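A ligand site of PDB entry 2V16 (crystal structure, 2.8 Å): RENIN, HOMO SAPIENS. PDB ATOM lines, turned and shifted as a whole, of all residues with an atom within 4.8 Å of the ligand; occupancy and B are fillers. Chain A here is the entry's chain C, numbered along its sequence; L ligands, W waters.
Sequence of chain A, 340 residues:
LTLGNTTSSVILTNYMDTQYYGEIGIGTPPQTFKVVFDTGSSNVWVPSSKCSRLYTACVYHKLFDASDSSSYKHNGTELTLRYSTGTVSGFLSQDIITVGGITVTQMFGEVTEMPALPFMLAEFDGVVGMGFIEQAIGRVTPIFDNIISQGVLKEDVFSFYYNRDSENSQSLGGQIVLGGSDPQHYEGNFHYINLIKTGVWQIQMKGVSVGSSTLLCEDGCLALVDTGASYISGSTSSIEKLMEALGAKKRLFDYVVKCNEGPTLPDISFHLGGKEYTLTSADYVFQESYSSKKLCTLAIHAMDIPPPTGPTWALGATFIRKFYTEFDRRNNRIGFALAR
The backbone carbonyl oxygen of Gly 228 sits close to a nitrogen (N2) of the ligand, at 3.2 Å.
OG1 of Thr 85 is in hydrogen-bond range of O3 of the ligand (3.1 Å).
The side-chain carboxylate (OD2) of Asp 226 is in salt-bridge range of a nitrogen (N2) of the ligand (3.2 Å).
The side-chain hydroxyl of Ser 230 sits at hydrogen-bond distance from an oxygen (O2) of the ligand (3.1 Å).
N2 of the ligand lies within salt-bridge range of OD1 of Asp 38.
The backbone NH (N) of Ser 84 lies within hydrogen-bond range of an oxygen (O5) of the ligand, 3.4 Å away.
An oxygen (O2) of the ligand sits at hydrogen-bond distance from the backbone NH (N) of Ser 230 (3.2 Å).
The backbone carbonyl oxygen (O) of Gly 40 lies close to the side-chain amide oxygen (OE1) of Gln 135 (3.1 Å).
OG of Ser 230 lies close to O of Thr 18.
OD2 of Asp 38 sits at hydrogen-bond distance from OG of Ser 41 (2.6 Å).
OD1 of Asp 38 sits at hydrogen-bond distance from N of Gly 40 (3.0 Å).
OE1 of Gln 19 lies close to O of Leu 121 (3.2 Å).
The side-chain hydroxyl (OH) of Tyr 162 lies within hydrogen-bond range of the backbone carbonyl oxygen (O) of Thr 227, at 2.5 Å.
The backbone carbonyl oxygen (O) of Thr 18 sits close to an oxygen (O2) of the ligand.
Residues that only touch the ligand: Gln 19 (3.4 Å), Tyr 20 (3.9 Å), Val 36 (3.4 Å), Gly 40 (3.4 Å), Ser 41 (3.4 Å), Arg 82 (3.1 Å), Tyr 83 (3.0 Å), Pro 118 (3.5 Å), Ala 122 (3.8 Å), Phe 124 (3.6 Å), Thr 227 (3.7 Å) and Ala 229 (3.5 Å).
Hydrophobic or aromatic side chains that line the ligand: Val 36, Tyr 83, Pro 118, Ala 122 and Phe 124.
Within 4 Å of the ligand: Thr 18, Gln 19, Tyr 20, Val 36, Asp 38, Gly 40, Ser 41, Arg 82, Tyr 83, Ser 84, Thr 85, Pro 118, Ala 122, Phe 124, Asp 226, Thr 227, Gly 228, Ala 229 and Ser 230.
The nearest printed residue that does not touch the ligand is Ile 305 (4.02 Å).
Water W2 bridges N2 of the ligand (3.1 Å) and OG of Ser 84 (3.3 Å).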
ATOM      1  N   THR A  18      -1.566 -25.168  -6.473  1.00  0.00           N
ATOM      2  CA  THR A  18      -1.682 -24.215  -7.482  1.00  0.00           C
ATOM      3  C   THR A  18      -0.471 -24.068  -8.329  1.00  0.00           C
ATOM      4  O   THR A  18      -0.340 -23.476  -9.399  1.00  0.00           O
ATOM      5  CB  THR A  18      -2.106 -22.883  -7.025  1.00  0.00           C
ATOM      6  OG1 THR A  18      -1.133 -22.495  -6.044  1.00  0.00           O
ATOM      7  CG2 THR A  18      -3.491 -22.871  -6.521  1.00  0.00           C
ATOM      8  N   GLN A  19       0.536 -24.642  -7.894  1.00  0.00           N
ATOM      9  CA  GLN A  19       1.827 -24.527  -8.642  1.00  0.00           C
ATOM     10  C   GLN A  19       2.687 -25.838  -8.455  1.00  0.00           C
ATOM     11  O   GLN A  19       3.025 -26.071  -7.355  1.00  0.00           O
ATOM     12  CB  GLN A  19       2.724 -23.504  -7.921  1.00  0.00           C
ATOM     13  CG  GLN A  19       2.873 -22.041  -8.501  1.00  0.00           C
ATOM     14  CD  GLN A  19       3.705 -21.554  -7.434  1.00  0.00           C
ATOM     15  OE1 GLN A  19       3.621 -20.397  -6.967  1.00  0.00           O
ATOM     16  NE2 GLN A  19       4.303 -22.669  -7.035  1.00  0.00           N
ATOM     17  N   TYR A  20       2.994 -26.558  -9.524  1.00  0.00           N
ATOM     18  CA  TYR A  20       3.618 -27.763  -9.689  1.00  0.00           C
ATOM     19  C   TYR A  20       4.903 -27.725 -10.448  1.00  0.00           C
ATOM     20  O   TYR A  20       4.816 -27.759 -11.562  1.00  0.00           O
ATOM     21  CB  TYR A  20       2.630 -28.808 -10.425  1.00  0.00           C
ATOM     22  CG  TYR A  20       1.440 -29.410  -9.799  1.00  0.00           C
ATOM     23  CD1 TYR A  20       0.243 -28.730  -9.679  1.00  0.00           C
ATOM     24  CD2 TYR A  20       1.365 -30.690  -9.268  1.00  0.00           C
ATOM     25  CE1 TYR A  20      -0.860 -29.175  -8.947  1.00  0.00           C
ATOM     26  CE2 TYR A  20       0.261 -31.171  -8.559  1.00  0.00           C
ATOM     27  CZ  TYR A  20      -0.902 -30.431  -8.364  1.00  0.00           C
ATOM     28  OH  TYR A  20      -2.062 -30.906  -7.792  1.00  0.00           O
ATOM     29  N   VAL A  36       8.241 -25.224 -13.801  1.00  0.00           N
ATOM     30  CA  VAL A  36       6.890 -25.714 -14.200  1.00  0.00           C
ATOM     31  C   VAL A  36       7.075 -26.342 -15.601  1.00  0.00           C
ATOM     32  O   VAL A  36       7.776 -25.809 -16.325  1.00  0.00           O
ATOM     33  CB  VAL A  36       5.796 -24.637 -14.356  1.00  0.00           C
ATOM     34  CG1 VAL A  36       4.280 -24.926 -14.591  1.00  0.00           C
ATOM     35  CG2 VAL A  36       5.579 -23.777 -13.130  1.00  0.00           C
ATOM     36  N   ASP A  38       5.315 -26.968 -18.605  1.00  0.00           N
ATOM     37  CA  ASP A  38       4.201 -26.341 -19.392  1.00  0.00           C
ATOM     38  C   ASP A  38       3.805 -26.779 -20.847  1.00  0.00           C
ATOM     39  O   ASP A  38       4.489 -26.444 -21.669  1.00  0.00           O
ATOM     40  CB  ASP A  38       4.419 -24.804 -19.596  1.00  0.00           C
ATOM     41  CG  ASP A  38       3.363 -23.793 -20.015  1.00  0.00           C
ATOM     42  OD1 ASP A  38       2.337 -23.977 -19.649  1.00  0.00           O
ATOM     43  OD2 ASP A  38       3.638 -22.650 -20.756  1.00  0.00           O
ATOM     44  N   GLY A  40       1.530 -25.222 -22.276  1.00  0.00           N
ATOM     45  CA  GLY A  40       0.867 -24.190 -22.868  1.00  0.00           C
ATOM     46  C   GLY A  40       1.861 -23.337 -23.679  1.00  0.00           C
ATOM     47  O   GLY A  40       1.576 -22.398 -24.337  1.00  0.00           O
ATOM     48  N   SER A  41       3.109 -23.604 -23.737  1.00  0.00           N
ATOM     49  CA  SER A  41       4.103 -22.739 -24.540  1.00  0.00           C
ATOM     50  C   SER A  41       5.294 -23.558 -24.913  1.00  0.00           C
ATOM     51  O   SER A  41       5.563 -24.725 -24.514  1.00  0.00           O
ATOM     52  CB  SER A  41       4.711 -21.504 -23.889  1.00  0.00           C
ATOM     53  OG  SER A  41       5.184 -22.053 -22.774  1.00  0.00           O
ATOM     54  N   LEU A  81       8.486 -12.994 -23.783  1.00  0.00           N
ATOM     55  CA  LEU A  81       7.511 -13.981 -23.714  1.00  0.00           C
ATOM     56  C   LEU A  81       6.259 -13.441 -23.183  1.00  0.00           C
ATOM     57  O   LEU A  81       6.171 -13.104 -22.051  1.00  0.00           O
ATOM     58  CB  LEU A  81       8.005 -15.139 -22.831  1.00  0.00           C
ATOM     59  CG  LEU A  81       9.401 -15.699 -23.219  1.00  0.00           C
ATOM     60  CD1 LEU A  81       9.884 -17.027 -22.672  1.00  0.00           C
ATOM     61  CD2 LEU A  81       9.291 -16.015 -24.572  1.00  0.00           C
ATOM     62  N   ARG A  82       5.173 -13.448 -23.917  1.00  0.00           N
ATOM     63  CA  ARG A  82       3.886 -13.013 -23.339  1.00  0.00           C
ATOM     64  C   ARG A  82       2.934 -14.090 -22.846  1.00  0.00           C
ATOM     65  O   ARG A  82       2.605 -15.011 -23.456  1.00  0.00           O
ATOM     66  CB  ARG A  82       3.195 -12.177 -24.214  1.00  0.00           C
ATOM     67  CG  ARG A  82       3.843 -10.860 -24.184  1.00  0.00           C
ATOM     68  CD  ARG A  82       3.479  -9.981 -25.342  1.00  0.00           C
ATOM     69  NE  ARG A  82       4.689  -9.511 -26.077  1.00  0.00           N
ATOM     70  CZ  ARG A  82       4.630  -8.590 -27.168  1.00  0.00           C
ATOM     71  NH1 ARG A  82       3.160  -8.155 -27.478  1.00  0.00           N
ATOM     72  NH2 ARG A  82       6.052  -8.069 -27.741  1.00  0.00           N
ATOM     73  N   TYR A  83       2.404 -14.049 -21.713  1.00  0.00           N
ATOM     74  CA  TYR A  83       1.641 -15.166 -21.437  1.00  0.00           C
ATOM     75  C   TYR A  83       0.222 -14.762 -21.016  1.00  0.00           C
ATOM     76  O   TYR A  83      -0.021 -13.691 -21.084  1.00  0.00           O
ATOM     77  CB  TYR A  83       2.337 -15.909 -20.238  1.00  0.00           C
ATOM     78  CG  TYR A  83       3.627 -16.603 -20.430  1.00  0.00           C
ATOM     79  CD1 TYR A  83       3.653 -17.837 -21.088  1.00  0.00           C
ATOM     80  CD2 TYR A  83       4.820 -16.045 -19.820  1.00  0.00           C
ATOM     81  CE1 TYR A  83       4.824 -18.448 -21.328  1.00  0.00           C
ATOM     82  CE2 TYR A  83       5.974 -16.670 -20.050  1.00  0.00           C
ATOM     83  CZ  TYR A  83       5.973 -17.915 -20.730  1.00  0.00           C
ATOM     84  OH  TYR A  83       7.034 -18.544 -20.924  1.00  0.00           O
ATOM     85  N   SER A  84      -0.707 -15.542 -20.500  1.00  0.00           N
ATOM     86  CA  SER A  84      -2.003 -15.322 -20.149  1.00  0.00           C
ATOM     87  C   SER A  84      -1.899 -14.195 -19.070  1.00  0.00           C
ATOM     88  O   SER A  84      -2.724 -13.242 -18.824  1.00  0.00           O
ATOM     89  CB  SER A  84      -2.155 -16.801 -19.440  1.00  0.00           C
ATOM     90  OG  SER A  84      -3.592 -17.207 -19.303  1.00  0.00           O
ATOM     91  N   THR A  85      -0.871 -14.434 -18.372  1.00  0.00           N
ATOM     92  CA  THR A  85      -0.708 -13.706 -17.226  1.00  0.00           C
ATOM     93  C   THR A  85       0.527 -12.995 -16.659  1.00  0.00           C
ATOM     94  O   THR A  85       0.375 -12.938 -15.457  1.00  0.00           O
ATOM     95  CB  THR A  85      -1.127 -14.730 -16.093  1.00  0.00           C
ATOM     96  OG1 THR A  85      -0.358 -15.896 -16.127  1.00  0.00           O
ATOM     97  CG2 THR A  85      -2.702 -14.832 -16.068  1.00  0.00           C
ATOM     98  N   PRO A 118       3.428 -11.570 -11.675  1.00  0.00           N
ATOM     99  CA  PRO A 118       3.200 -12.474 -10.732  1.00  0.00           C
ATOM    100  C   PRO A 118       4.320 -13.120 -10.214  1.00  0.00           C
ATOM    101  O   PRO A 118       4.338 -13.911  -9.362  1.00  0.00           O
ATOM    102  CB  PRO A 118       2.389 -13.466 -11.621  1.00  0.00           C
ATOM    103  CG  PRO A 118       2.820 -13.386 -12.962  1.00  0.00           C
ATOM    104  CD  PRO A 118       3.375 -12.045 -13.005  1.00  0.00           C
ATOM    105  N   PHE A 119       5.334 -12.971 -10.839  1.00  0.00           N
ATOM    106  CA  PHE A 119       6.555 -13.718 -10.467  1.00  0.00           C
ATOM    107  C   PHE A 119       7.140 -13.663  -9.051  1.00  0.00           C
ATOM    108  O   PHE A 119       7.837 -14.446  -8.778  1.00  0.00           O
ATOM    109  CB  PHE A 119       7.605 -13.555 -11.490  1.00  0.00           C
ATOM    110  CG  PHE A 119       7.089 -14.065 -12.765  1.00  0.00           C
ATOM    111  CD1 PHE A 119       7.034 -15.402 -13.003  1.00  0.00           C
ATOM    112  CD2 PHE A 119       6.765 -13.243 -13.851  1.00  0.00           C
ATOM    113  CE1 PHE A 119       6.517 -15.783 -14.231  1.00  0.00           C
ATOM    114  CE2 PHE A 119       6.293 -13.658 -15.170  1.00  0.00           C
ATOM    115  CZ  PHE A 119       6.096 -14.949 -15.280  1.00  0.00           C
ATOM    116  N   LEU A 121       5.449 -14.298  -6.466  1.00  0.00           N
ATOM    117  CA  LEU A 121       4.630 -15.223  -5.914  1.00  0.00           C
ATOM    118  C   LEU A 121       4.730 -16.583  -6.471  1.00  0.00           C
ATOM    119  O   LEU A 121       3.823 -17.350  -6.146  1.00  0.00           O
ATOM    120  CB  LEU A 121       3.273 -14.936  -6.558  1.00  0.00           C
ATOM    121  CG  LEU A 121       2.494 -13.685  -6.058  1.00  0.00           C
ATOM    122  CD1 LEU A 121       1.056 -14.031  -6.364  1.00  0.00           C
ATOM    123  CD2 LEU A 121       2.749 -13.277  -4.514  1.00  0.00           C
ATOM    124  N   ALA A 122       5.723 -16.804  -7.330  1.00  0.00           N
ATOM    125  CA  ALA A 122       5.949 -18.030  -7.890  1.00  0.00           C
ATOM    126  C   ALA A 122       6.887 -18.841  -7.151  1.00  0.00           C
ATOM    127  O   ALA A 122       7.867 -18.496  -6.999  1.00  0.00           O
ATOM    128  CB  ALA A 122       6.639 -17.711  -9.103  1.00  0.00           C
ATOM    129  N   PHE A 124       8.544 -21.352  -8.375  1.00  0.00           N
ATOM    130  CA  PHE A 124       9.385 -21.864  -9.287  1.00  0.00           C
ATOM    131  C   PHE A 124      10.238 -20.752  -9.819  1.00  0.00           C
ATOM    132  O   PHE A 124       9.952 -19.644  -9.554  1.00  0.00           O
ATOM    133  CB  PHE A 124       8.406 -22.575 -10.200  1.00  0.00           C
ATOM    134  CG  PHE A 124       7.520 -21.709 -11.012  1.00  0.00           C
ATOM    135  CD1 PHE A 124       7.923 -21.017 -12.166  1.00  0.00           C
ATOM    136  CD2 PHE A 124       6.189 -21.590 -10.738  1.00  0.00           C
ATOM    137  CE1 PHE A 124       7.103 -20.163 -12.962  1.00  0.00           C
ATOM    138  CE2 PHE A 124       5.400 -20.729 -11.454  1.00  0.00           C
ATOM    139  CZ  PHE A 124       5.813 -20.006 -12.605  1.00  0.00           C
ATOM    140  N   VAL A 127      10.272 -21.711 -16.556  1.00  0.00           N
ATOM    141  CA  VAL A 127       9.455 -22.485 -17.286  1.00  0.00           C
ATOM    142  C   VAL A 127      10.122 -23.388 -18.435  1.00  0.00           C
ATOM    143  O   VAL A 127      11.055 -22.955 -19.092  1.00  0.00           O
ATOM    144  CB  VAL A 127       8.487 -21.425 -17.784  1.00  0.00           C
ATOM    145  CG1 VAL A 127       8.266 -21.603 -19.203  1.00  0.00           C
ATOM    146  CG2 VAL A 127       7.187 -21.838 -17.368  1.00  0.00           C
ATOM    147  N   GLN A 135       4.703 -22.746 -31.657  1.00  0.00           N
ATOM    148  CA  GLN A 135       4.316 -21.661 -30.771  1.00  0.00           C
ATOM    149  C   GLN A 135       5.483 -21.023 -29.946  1.00  0.00           C
ATOM    150  O   GLN A 135       5.484 -20.408 -28.959  1.00  0.00           O
ATOM    151  CB  GLN A 135       2.873 -22.098 -30.171  1.00  0.00           C
ATOM    152  CG  GLN A 135       3.035 -22.852 -28.911  1.00  0.00           C
ATOM    153  CD  GLN A 135       1.798 -23.509 -28.174  1.00  0.00           C
ATOM    154  OE1 GLN A 135       0.937 -22.779 -27.376  1.00  0.00           O
ATOM    155  NE2 GLN A 135       1.635 -24.952 -28.259  1.00  0.00           N
ATOM    156  N   ILE A 137       8.420 -18.769 -29.598  1.00  0.00           N
ATOM    157  CA  ILE A 137       8.783 -17.448 -29.942  1.00  0.00           C
ATOM    158  C   ILE A 137      10.187 -17.567 -30.270  1.00  0.00           C
ATOM    159  O   ILE A 137      10.947 -18.405 -29.641  1.00  0.00           O
ATOM    160  CB  ILE A 137       8.591 -16.835 -28.673  1.00  0.00           C
ATOM    161  CG1 ILE A 137       7.248 -16.277 -28.841  1.00  0.00           C
ATOM    162  CG2 ILE A 137       9.634 -15.828 -28.529  1.00  0.00           C
ATOM    163  CD1 ILE A 137       7.450 -14.939 -28.284  1.00  0.00           C
ATOM    164  N   TYR A 162      -0.670 -35.081 -11.598  1.00  0.00           N
ATOM    165  CA  TYR A 162      -0.652 -34.083 -10.682  1.00  0.00           C
ATOM    166  C   TYR A 162      -1.343 -34.659  -9.346  1.00  0.00           C
ATOM    167  O   TYR A 162      -2.413 -35.253  -9.294  1.00  0.00           O
ATOM    168  CB  TYR A 162      -1.331 -32.859 -11.090  1.00  0.00           C
ATOM    169  CG  TYR A 162      -0.580 -31.955 -11.907  1.00  0.00           C
ATOM    170  CD1 TYR A 162       0.755 -32.237 -12.112  1.00  0.00           C
ATOM    171  CD2 TYR A 162      -1.120 -30.813 -12.452  1.00  0.00           C
ATOM    172  CE1 TYR A 162       1.435 -31.399 -13.006  1.00  0.00           C
ATOM    173  CE2 TYR A 162      -0.320 -29.959 -13.208  1.00  0.00           C
ATOM    174  CZ  TYR A 162       0.985 -30.201 -13.564  1.00  0.00           C
ATOM    175  OH  TYR A 162       1.738 -29.401 -14.311  1.00  0.00           O
ATOM    176  N   LEU A 224      -7.734 -25.900 -24.408  1.00  0.00           N
ATOM    177  CA  LEU A 224      -6.352 -26.138 -24.578  1.00  0.00           C
ATOM    178  C   LEU A 224      -6.113 -26.921 -23.381  1.00  0.00           C
ATOM    179  O   LEU A 224      -6.774 -26.607 -22.483  1.00  0.00           O
ATOM    180  CB  LEU A 224      -5.704 -24.838 -24.483  1.00  0.00           C
ATOM    181  CG  LEU A 224      -4.275 -24.854 -23.842  1.00  0.00           C
ATOM    182  CD1 LEU A 224      -3.354 -24.633 -24.989  1.00  0.00           C
ATOM    183  CD2 LEU A 224      -3.899 -23.508 -23.199  1.00  0.00           C
ATOM    184  N   ASP A 226      -3.550 -27.593 -20.625  1.00  0.00           N
ATOM    185  CA  ASP A 226      -2.306 -26.910 -20.196  1.00  0.00           C
ATOM    186  C   ASP A 226      -1.865 -27.204 -18.862  1.00  0.00           C
ATOM    187  O   ASP A 226      -2.418 -26.754 -18.071  1.00  0.00           O
ATOM    188  CB  ASP A 226      -2.726 -25.426 -20.286  1.00  0.00           C
ATOM    189  CG  ASP A 226      -2.012 -24.204 -19.865  1.00  0.00           C
ATOM    190  OD1 ASP A 226      -2.577 -23.217 -19.627  1.00  0.00           O
ATOM    191  OD2 ASP A 226      -0.831 -24.176 -19.827  1.00  0.00           O
ATOM    192  N   THR A 227      -0.793 -27.875 -18.720  1.00  0.00           N
ATOM    193  CA  THR A 227      -0.184 -28.275 -17.487  1.00  0.00           C
ATOM    194  C   THR A 227       0.411 -27.228 -16.613  1.00  0.00           C
ATOM    195  O   THR A 227       0.589 -27.530 -15.466  1.00  0.00           O
ATOM    196  CB  THR A 227       0.923 -29.302 -17.785  1.00  0.00           C
ATOM    197  OG1 THR A 227       2.085 -28.638 -18.220  1.00  0.00           O
ATOM    198  CG2 THR A 227       0.414 -30.393 -18.648  1.00  0.00           C
ATOM    199  N   GLY A 228       0.703 -26.133 -17.177  1.00  0.00           N
ATOM    200  CA  GLY A 228       1.342 -25.046 -16.611  1.00  0.00           C
ATOM    201  C   GLY A 228       0.460 -23.971 -16.084  1.00  0.00           C
ATOM    202  O   GLY A 228       0.816 -22.948 -15.696  1.00  0.00           O
ATOM    203  N   ALA A 229      -0.762 -24.252 -16.081  1.00  0.00           N
ATOM    204  CA  ALA A 229      -1.972 -23.575 -15.579  1.00  0.00           C
ATOM    205  C   ALA A 229      -2.615 -24.292 -14.366  1.00  0.00           C
ATOM    206  O   ALA A 229      -2.847 -25.463 -14.219  1.00  0.00           O
ATOM    207  CB  ALA A 229      -3.033 -23.640 -16.614  1.00  0.00           C
ATOM    208  N   SER A 230      -2.993 -23.557 -13.474  1.00  0.00           N
ATOM    209  CA  SER A 230      -3.495 -24.038 -12.329  1.00  0.00           C
ATOM    210  C   SER A 230      -4.882 -24.218 -12.268  1.00  0.00           C
ATOM    211  O   SER A 230      -5.309 -24.894 -11.359  1.00  0.00           O
ATOM    212  CB  SER A 230      -2.969 -23.344 -10.987  1.00  0.00           C
ATOM    213  OG  SER A 230      -2.538 -22.048 -11.046  1.00  0.00           O
ATOM    214  N   ILE A 305      -7.339 -15.785 -23.761  1.00  0.00           N
ATOM    215  CA  ILE A 305      -6.121 -16.016 -24.428  1.00  0.00           C
ATOM    216  C   ILE A 305      -6.664 -15.747 -25.838  1.00  0.00           C
ATOM    217  O   ILE A 305      -7.707 -16.207 -26.395  1.00  0.00           O
ATOM    218  CB  ILE A 305      -5.890 -17.444 -24.185  1.00  0.00           C
ATOM    219  CG1 ILE A 305      -5.644 -17.837 -22.836  1.00  0.00           C
ATOM    220  CG2 ILE A 305      -5.190 -18.212 -25.271  1.00  0.00           C
ATOM    221  CD1 ILE A 305      -6.608 -18.980 -22.696  1.00  0.00           C
HETATM  222  C1  LIG L   1       0.666 -25.215 -12.581  1.00  0.00           C
HETATM  223  O1  LIG L   1       1.769 -24.191 -12.349  1.00  0.00           O
HETATM  224  C2  LIG L   1       1.270 -22.862 -12.521  1.00  0.00           C
HETATM  225  O2  LIG L   1       0.025 -22.738 -12.635  1.00  0.00           O
HETATM  226  C3  LIG L   1       2.099 -21.638 -12.640  1.00  0.00           C
HETATM  227  C4  LIG L   1       1.525 -20.923 -11.438  1.00  0.00           C
HETATM  228  C5  LIG L   1       2.031 -19.536 -11.367  1.00  0.00           C
HETATM  229  C6  LIG L   1       2.473 -18.929 -10.136  1.00  0.00           C
HETATM  230  C7  LIG L   1       3.022 -17.513 -10.229  1.00  0.00           C
HETATM  231  C8  LIG L   1       3.188 -16.823 -11.426  1.00  0.00           C
HETATM  232  C9  LIG L   1       2.846 -17.447 -12.633  1.00  0.00           C
HETATM  233  C10 LIG L   1       2.290 -18.865 -12.615  1.00  0.00           C
HETATM  234  N1  LIG L   1       1.846 -19.626 -13.845  1.00  0.00           N
HETATM  235  C11 LIG L   1       1.474 -20.993 -13.781  1.00  0.00           C
HETATM  236  C12 LIG L   1       1.728 -18.974 -15.090  1.00  0.00           C
HETATM  237  O3  LIG L   1       1.954 -17.757 -15.179  1.00  0.00           O
HETATM  238  C13 LIG L   1       1.416 -19.782 -16.354  1.00  0.00           C
HETATM  239  C14 LIG L   1       2.480 -19.457 -17.289  1.00  0.00           C
HETATM  240  C15 LIG L   1       3.831 -19.646 -16.730  1.00  0.00           C
HETATM  241  C16 LIG L   1       2.455 -18.002 -17.802  1.00  0.00           C
HETATM  242  C17 LIG L   1       2.357 -20.342 -18.416  1.00  0.00           C
HETATM  243  C18 LIG L   1       0.965 -20.149 -19.006  1.00  0.00           C
HETATM  244  N2  LIG L   1       0.167 -21.411 -18.481  1.00  0.00           N
HETATM  245  C19 LIG L   1       0.957 -20.220 -20.531  1.00  0.00           C
HETATM  246  O4  LIG L   1       1.012 -21.701 -20.630  1.00  0.00           O
HETATM  247  C20 LIG L   1      -0.494 -19.631 -20.912  1.00  0.00           C
HETATM  248  C21 LIG L   1      -0.631 -19.795 -22.420  1.00  0.00           C
HETATM  249  C22 LIG L   1      -2.146 -19.815 -22.771  1.00  0.00           C
HETATM  250  C23 LIG L   1       0.346 -18.773 -23.063  1.00  0.00           C
HETATM  251  O5  LIG L   1       0.837 -17.917 -22.423  1.00  0.00           O
HETATM  252  N3  LIG L   1       0.682 -18.844 -24.287  1.00  0.00           N
HETATM  253  C24 LIG L   1       1.780 -18.141 -24.910  1.00  0.00           C
HETATM  254  C25 LIG L   1       2.901 -18.373 -24.095  1.00  0.00           C
HETATM  255  C26 LIG L   1       4.052 -18.402 -25.019  1.00  0.00           C
HETATM  256  C27 LIG L   1       4.092 -16.863 -25.441  1.00  0.00           C
HETATM  257  O   HOH W   1       6.443 -20.377 -26.079  1.00  0.00           O
HETATM  258  O   HOH W   2      -1.362 -18.933 -17.548  1.00  0.00           O
